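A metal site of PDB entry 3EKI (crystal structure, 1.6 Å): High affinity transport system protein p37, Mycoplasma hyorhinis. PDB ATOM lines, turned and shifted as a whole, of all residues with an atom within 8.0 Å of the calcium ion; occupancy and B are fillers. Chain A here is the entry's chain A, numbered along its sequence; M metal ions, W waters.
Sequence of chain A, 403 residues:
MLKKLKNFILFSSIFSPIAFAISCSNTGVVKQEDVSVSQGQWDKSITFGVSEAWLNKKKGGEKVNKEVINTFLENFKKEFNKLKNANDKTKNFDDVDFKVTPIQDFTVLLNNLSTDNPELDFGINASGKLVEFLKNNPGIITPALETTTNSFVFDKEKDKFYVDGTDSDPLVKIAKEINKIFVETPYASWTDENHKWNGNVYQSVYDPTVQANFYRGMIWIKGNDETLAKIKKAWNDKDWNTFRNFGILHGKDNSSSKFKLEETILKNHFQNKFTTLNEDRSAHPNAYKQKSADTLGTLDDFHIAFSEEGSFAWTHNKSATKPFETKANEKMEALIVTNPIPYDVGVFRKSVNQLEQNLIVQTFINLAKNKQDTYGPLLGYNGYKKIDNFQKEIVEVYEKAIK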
ATOM      1  N   TRP A  42     -11.587  -3.401 -31.267  1.00  0.00           N
ATOM      2  CA  TRP A  42     -12.888  -3.826 -30.737  1.00  0.00           C
ATOM      3  C   TRP A  42     -12.856  -5.317 -30.520  1.00  0.00           C
ATOM      4  O   TRP A  42     -12.456  -6.117 -31.370  1.00  0.00           O
ATOM      5  CB  TRP A  42     -14.020  -3.466 -31.700  1.00  0.00           C
ATOM      6  CG  TRP A  42     -15.387  -3.697 -31.115  1.00  0.00           C
ATOM      7  CD1 TRP A  42     -16.149  -4.812 -31.198  1.00  0.00           C
ATOM      8  CD2 TRP A  42     -16.106  -2.714 -30.345  1.00  0.00           C
ATOM      9  NE1 TRP A  42     -17.329  -4.606 -30.534  1.00  0.00           N
ATOM     10  CE2 TRP A  42     -17.332  -3.326 -30.004  1.00  0.00           C
ATOM     11  CE3 TRP A  42     -15.848  -1.393 -29.935  1.00  0.00           C
ATOM     12  CZ2 TRP A  42     -18.278  -2.639 -29.243  1.00  0.00           C
ATOM     13  CZ3 TRP A  42     -16.805  -0.734 -29.189  1.00  0.00           C
ATOM     14  CH2 TRP A  42     -18.021  -1.341 -28.840  1.00  0.00           C
ATOM     15  N   ASP A  43     -13.282  -5.787 -29.349  1.00  0.00           N
ATOM     16  CA  ASP A  43     -13.239  -7.203 -29.061  1.00  0.00           C
ATOM     17  C   ASP A  43     -14.656  -7.687 -28.827  1.00  0.00           C
ATOM     18  O   ASP A  43     -15.295  -7.172 -27.894  1.00  0.00           O
ATOM     19  CB  ASP A  43     -12.361  -7.449 -27.833  1.00  0.00           C
ATOM     20  CG  ASP A  43     -12.069  -8.889 -27.565  1.00  0.00           C
ATOM     21  OD1 ASP A  43     -12.638  -9.764 -28.277  1.00  0.00           O
ATOM     22  OD2 ASP A  43     -11.263  -9.198 -26.657  1.00  0.00           O
ATOM     23  N   LYS A  44     -15.167  -8.598 -29.632  1.00  0.00           N
ATOM     24  CA  LYS A  44     -16.562  -9.014 -29.508  1.00  0.00           C
ATOM     25  C   LYS A  44     -16.805  -9.974 -28.373  1.00  0.00           C
ATOM     26  O   LYS A  44     -17.957 -10.373 -28.112  1.00  0.00           O
ATOM     27  CB  LYS A  44     -17.037  -9.637 -30.832  1.00  0.00           C
ATOM     28  CG  LYS A  44     -16.332 -10.966 -31.109  1.00  0.00           C
ATOM     29  CD  LYS A  44     -16.593 -11.480 -32.524  1.00  0.00           C
ATOM     30  CE  LYS A  44     -15.950 -12.841 -32.721  1.00  0.00           C
ATOM     31  NZ  LYS A  44     -15.446 -13.008 -34.113  1.00  0.00           N
ATOM     32  N   SER A  45     -15.775 -10.350 -27.641  1.00  0.00           N
ATOM     33  CA  SER A  45     -15.863 -11.231 -26.488  1.00  0.00           C
ATOM     34  C   SER A  45     -15.091 -10.566 -25.348  1.00  0.00           C
ATOM     35  O   SER A  45     -13.887 -10.322 -25.486  1.00  0.00           O
ATOM     36  CB  SER A  45     -15.284 -12.604 -26.789  1.00  0.00           C
ATOM     37  OG  SER A  45     -15.132 -13.401 -25.617  1.00  0.00           O
ATOM     38  N   ILE A  46     -15.758 -10.237 -24.241  1.00  0.00           N
ATOM     39  CA  ILE A  46     -15.058  -9.638 -23.117  1.00  0.00           C
ATOM     40  C   ILE A  46     -15.121 -10.627 -21.955  1.00  0.00           C
ATOM     41  O   ILE A  46     -16.213 -11.072 -21.635  1.00  0.00           O
ATOM     42  CB  ILE A  46     -15.664  -8.275 -22.803  1.00  0.00           C
ATOM     43  CG1 ILE A  46     -15.394  -7.199 -23.862  1.00  0.00           C
ATOM     44  CG2 ILE A  46     -15.218  -7.769 -21.424  1.00  0.00           C
ATOM     45  CD1 ILE A  46     -13.962  -6.691 -23.827  1.00  0.00           C
ATOM     46  N   THR A  47     -13.969 -10.940 -21.413  1.00  0.00           N
ATOM     47  CA  THR A  47     -13.844 -11.838 -20.278  1.00  0.00           C
ATOM     48  C   THR A  47     -13.302 -11.094 -19.054  1.00  0.00           C
ATOM     49  O   THR A  47     -12.201 -10.541 -19.135  1.00  0.00           O
ATOM     50  CB  THR A  47     -12.906 -13.014 -20.623  1.00  0.00           C
ATOM     51  OG1 THR A  47     -13.455 -13.754 -21.725  1.00  0.00           O
ATOM     52  CG2 THR A  47     -12.795 -13.970 -19.450  1.00  0.00           C
ATOM     53  N   PHE A  48     -14.044 -11.083 -17.967  1.00  0.00           N
ATOM     54  CA  PHE A  48     -13.627 -10.564 -16.677  1.00  0.00           C
ATOM     55  C   PHE A  48     -12.952 -11.633 -15.817  1.00  0.00           C
ATOM     56  O   PHE A  48     -13.447 -12.758 -15.661  1.00  0.00           O
ATOM     57  CB  PHE A  48     -14.843 -10.018 -15.926  1.00  0.00           C
ATOM     58  CG  PHE A  48     -15.591  -8.870 -16.595  1.00  0.00           C
ATOM     59  CD1 PHE A  48     -14.984  -8.019 -17.500  1.00  0.00           C
ATOM     60  CD2 PHE A  48     -16.919  -8.664 -16.282  1.00  0.00           C
ATOM     61  CE1 PHE A  48     -15.727  -6.983 -18.077  1.00  0.00           C
ATOM     62  CE2 PHE A  48     -17.656  -7.635 -16.839  1.00  0.00           C
ATOM     63  CZ  PHE A  48     -17.038  -6.778 -17.725  1.00  0.00           C
ATOM     64  N   VAL A  96     -21.272  -7.546 -28.259  1.00  0.00           N
ATOM     65  CA  VAL A  96     -20.300  -8.144 -27.366  1.00  0.00           C
ATOM     66  C   VAL A  96     -20.927  -9.130 -26.394  1.00  0.00           C
ATOM     67  O   VAL A  96     -21.985  -8.855 -25.821  1.00  0.00           O
ATOM     68  CB  VAL A  96     -19.597  -7.019 -26.572  1.00  0.00           C
ATOM     69  CG1 VAL A  96     -18.541  -7.601 -25.658  1.00  0.00           C
ATOM     70  CG2 VAL A  96     -18.967  -6.044 -27.563  1.00  0.00           C
ATOM     71  N   ASP A  97     -20.258 -10.260 -26.245  1.00  0.00           N
ATOM     72  CA  ASP A  97     -20.574 -11.272 -25.239  1.00  0.00           C
ATOM     73  C   ASP A  97     -19.679 -11.094 -24.008  1.00  0.00           C
ATOM     74  O   ASP A  97     -18.509 -10.723 -24.146  1.00  0.00           O
ATOM     75  CB  ASP A  97     -20.335 -12.689 -25.756  1.00  0.00           C
ATOM     76  CG  ASP A  97     -20.776 -13.745 -24.764  1.00  0.00           C
ATOM     77  OD1 ASP A  97     -21.832 -13.509 -24.136  1.00  0.00           O
ATOM     78  OD2 ASP A  97     -20.086 -14.767 -24.597  1.00  0.00           O
ATOM     79  N   LYS A  99     -18.108 -12.824 -20.383  1.00  0.00           N
ATOM     80  CA  LYS A  99     -17.769 -14.076 -19.745  1.00  0.00           C
ATOM     81  C   LYS A  99     -16.919 -13.765 -18.504  1.00  0.00           C
ATOM     82  O   LYS A  99     -16.477 -12.635 -18.393  1.00  0.00           O
ATOM     83  CB  LYS A  99     -17.011 -15.020 -20.674  1.00  0.00           C
ATOM     84  CG  LYS A  99     -17.708 -15.303 -21.993  1.00  0.00           C
ATOM     85  CD  LYS A  99     -16.912 -16.341 -22.774  1.00  0.00           C
ATOM     86  CE  LYS A  99     -16.577 -15.861 -24.180  1.00  0.00           C
ATOM     87  NZ  LYS A  99     -15.501 -16.700 -24.786  1.00  0.00           N
ATOM     88  N   ASN A 117      -3.568 -10.415 -23.867  1.00  0.00           N
ATOM     89  CA  ASN A 117      -4.132 -11.570 -24.540  1.00  0.00           C
ATOM     90  C   ASN A 117      -5.648 -11.442 -24.484  1.00  0.00           C
ATOM     91  O   ASN A 117      -6.171 -11.269 -23.373  1.00  0.00           O
ATOM     92  CB  ASN A 117      -3.662 -12.863 -23.880  1.00  0.00           C
ATOM     93  CG  ASN A 117      -4.097 -14.136 -24.542  1.00  0.00           C
ATOM     94  OD1 ASN A 117      -5.265 -14.390 -24.810  1.00  0.00           O
ATOM     95  ND2 ASN A 117      -3.137 -15.015 -24.840  1.00  0.00           N
ATOM     96  N   PRO A 118      -6.368 -11.502 -25.592  1.00  0.00           N
ATOM     97  CA  PRO A 118      -7.821 -11.347 -25.545  1.00  0.00           C
ATOM     98  C   PRO A 118      -8.586 -12.372 -24.738  1.00  0.00           C
ATOM     99  O   PRO A 118      -9.802 -12.234 -24.539  1.00  0.00           O
ATOM    100  CB  PRO A 118      -8.246 -11.445 -27.020  1.00  0.00           C
ATOM    101  CG  PRO A 118      -7.011 -11.120 -27.785  1.00  0.00           C
ATOM    102  CD  PRO A 118      -5.852 -11.641 -26.968  1.00  0.00           C
ATOM    103  N   GLU A 119      -7.980 -13.439 -24.216  1.00  0.00           N
ATOM    104  CA  GLU A 119      -8.668 -14.372 -23.355  1.00  0.00           C
ATOM    105  C   GLU A 119      -8.963 -13.775 -21.978  1.00  0.00           C
ATOM    106  O   GLU A 119      -9.812 -14.329 -21.274  1.00  0.00           O
ATOM    107  CB  GLU A 119      -7.883 -15.677 -23.147  1.00  0.00           C
ATOM    108  CG  GLU A 119      -6.890 -15.681 -22.007  1.00  0.00           C
ATOM    109  CD  GLU A 119      -5.687 -16.562 -22.297  1.00  0.00           C
ATOM    110  OE1 GLU A 119      -5.873 -17.616 -22.944  1.00  0.00           O
ATOM    111  OE2 GLU A 119      -4.579 -16.170 -21.876  1.00  0.00           O
ATOM    112  N   LEU A 120      -8.308 -12.678 -21.620  1.00  0.00           N
ATOM    113  CA  LEU A 120      -8.557 -11.991 -20.348  1.00  0.00           C
ATOM    114  C   LEU A 120      -8.441 -10.490 -20.569  1.00  0.00           C
ATOM    115  O   LEU A 120      -7.374  -9.942 -20.828  1.00  0.00           O
ATOM    116  CB  LEU A 120      -7.589 -12.435 -19.239  1.00  0.00           C
ATOM    117  CG  LEU A 120      -7.721 -11.651 -17.927  1.00  0.00           C
ATOM    118  CD1 LEU A 120      -9.072 -11.926 -17.287  1.00  0.00           C
ATOM    119  CD2 LEU A 120      -6.572 -12.017 -17.014  1.00  0.00           C
ATOM    120  N   ASP A 121      -9.585  -9.815 -20.485  1.00  0.00           N
ATOM    121  CA  ASP A 121      -9.680  -8.418 -20.888  1.00  0.00           C
ATOM    122  C   ASP A 121      -9.735  -7.403 -19.739  1.00  0.00           C
ATOM    123  O   ASP A 121      -9.372  -6.241 -19.938  1.00  0.00           O
ATOM    124  CB  ASP A 121     -10.931  -8.257 -21.749  1.00  0.00           C
ATOM    125  CG  ASP A 121     -10.978  -9.219 -22.924  1.00  0.00           C
ATOM    126  OD1 ASP A 121     -11.792 -10.166 -22.939  1.00  0.00           O
ATOM    127  OD2 ASP A 121     -10.111  -9.074 -23.818  1.00  0.00           O
ATOM    128  N   PHE A 122     -10.227  -7.826 -18.578  1.00  0.00           N
ATOM    129  CA  PHE A 122     -10.460  -6.862 -17.518  1.00  0.00           C
ATOM    130  C   PHE A 122     -10.508  -7.570 -16.175  1.00  0.00           C
ATOM    131  O   PHE A 122     -10.887  -8.723 -16.057  1.00  0.00           O
ATOM    132  CB  PHE A 122     -11.778  -6.143 -17.766  1.00  0.00           C
ATOM    133  CG  PHE A 122     -12.344  -5.207 -16.743  1.00  0.00           C
ATOM    134  CD1 PHE A 122     -12.051  -3.858 -16.793  1.00  0.00           C
ATOM    135  CD2 PHE A 122     -13.182  -5.693 -15.744  1.00  0.00           C
ATOM    136  CE1 PHE A 122     -12.587  -2.991 -15.846  1.00  0.00           C
ATOM    137  CE2 PHE A 122     -13.718  -4.847 -14.785  1.00  0.00           C
ATOM    138  CZ  PHE A 122     -13.408  -3.504 -14.887  1.00  0.00           C
ATOM    139  N   ARG A 349      -6.658  -4.790 -20.082  1.00  0.00           N
ATOM    140  CA  ARG A 349      -5.519  -4.997 -20.973  1.00  0.00           C
ATOM    141  C   ARG A 349      -5.503  -3.820 -21.969  1.00  0.00           C
ATOM    142  O   ARG A 349      -6.513  -3.213 -22.314  1.00  0.00           O
ATOM    143  CB  ARG A 349      -5.514  -6.351 -21.637  1.00  0.00           C
ATOM    144  CG  ARG A 349      -6.668  -6.580 -22.596  1.00  0.00           C
ATOM    145  CD  ARG A 349      -6.601  -7.902 -23.350  1.00  0.00           C
ATOM    146  NE  ARG A 349      -7.685  -7.992 -24.330  1.00  0.00           N
ATOM    147  CZ  ARG A 349      -7.713  -7.584 -25.573  1.00  0.00           C
ATOM    148  NH1 ARG A 349      -6.654  -7.004 -26.107  1.00  0.00           N
ATOM    149  NH2 ARG A 349      -8.808  -7.751 -26.312  1.00  0.00           N
ATOM    150  N   VAL A 352      -7.691  -3.241 -25.525  1.00  0.00           N
ATOM    151  CA  VAL A 352      -9.134  -3.151 -25.693  1.00  0.00           C
ATOM    152  C   VAL A 352      -9.497  -1.780 -26.210  1.00  0.00           C
ATOM    153  O   VAL A 352      -9.034  -0.745 -25.687  1.00  0.00           O
ATOM    154  CB  VAL A 352      -9.898  -3.397 -24.364  1.00  0.00           C
ATOM    155  CG1 VAL A 352     -11.356  -3.053 -24.568  1.00  0.00           C
ATOM    156  CG2 VAL A 352      -9.678  -4.811 -23.900  1.00  0.00           C
ATOM    157  N   GLU A 356     -14.942   0.924 -26.368  1.00  0.00           N
ATOM    158  CA  GLU A 356     -15.458  -0.249 -25.649  1.00  0.00           C
ATOM    159  C   GLU A 356     -15.179  -0.137 -24.152  1.00  0.00           C
ATOM    160  O   GLU A 356     -16.062  -0.448 -23.340  1.00  0.00           O
ATOM    161  CB  GLU A 356     -14.868  -1.518 -26.255  1.00  0.00           C
ATOM    162  CG  GLU A 356     -15.576  -2.794 -25.811  1.00  0.00           C
ATOM    163  CD  GLU A 356     -15.125  -4.034 -26.548  1.00  0.00           C
ATOM    164  OE1 GLU A 356     -14.106  -3.931 -27.260  1.00  0.00           O
ATOM    165  OE2 GLU A 356     -15.772  -5.096 -26.425  1.00  0.00           O
HETATM  166 CA    CA M   1     -11.636 -10.961 -25.061  1.00  0.00          CA
HETATM  167  O   HOH W   1     -13.017 -13.030 -24.247  1.00  0.00           O
HETATM  168  O   HOH W   2     -11.808 -12.367 -27.167  1.00  0.00           O
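O of Asp 121 lies within hydrogen-bond range of N of Arg 349, 3.1 Å away.
N of Asp 121 lies within hydrogen-bond range of O of Thr 47.
OD2 of Asp 43 lies close to NH2 of Arg 349 (2.9 Å).
OG of Ser 45 sits close to NZ of Lys 99, at 3.4 Å.
The backbone NH (N) of Asp 43 sits at hydrogen-bond distance from the side-chain carboxylate (OE1) of Glu 356 (2.9 Å).
Within 4 Å of the calcium ion: Asp 43, Ser 45, Pro 118 and Asp 121.
The calcium ion is bound by the side-chain carboxylate (OD1) of Asp 121 (2.3 Å), the backbone carbonyl oxygen (O) of Pro 118 (2.3 Å), the backbone carbonyl oxygen (O) of Ser 45 (2.4 Å), the side-chain carboxylate (OD2) of Asp 43 (2.4 Å), water W2 (2.5 Å), water W1 (2.6 Å) and the side-chain carboxylate (OD2) of Asp 121 (2.7 Å).
The calcium ion has seven donor atoms within binding distance.
Water W1 bridges OG of Ser 45 and OG1 of Thr 47.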
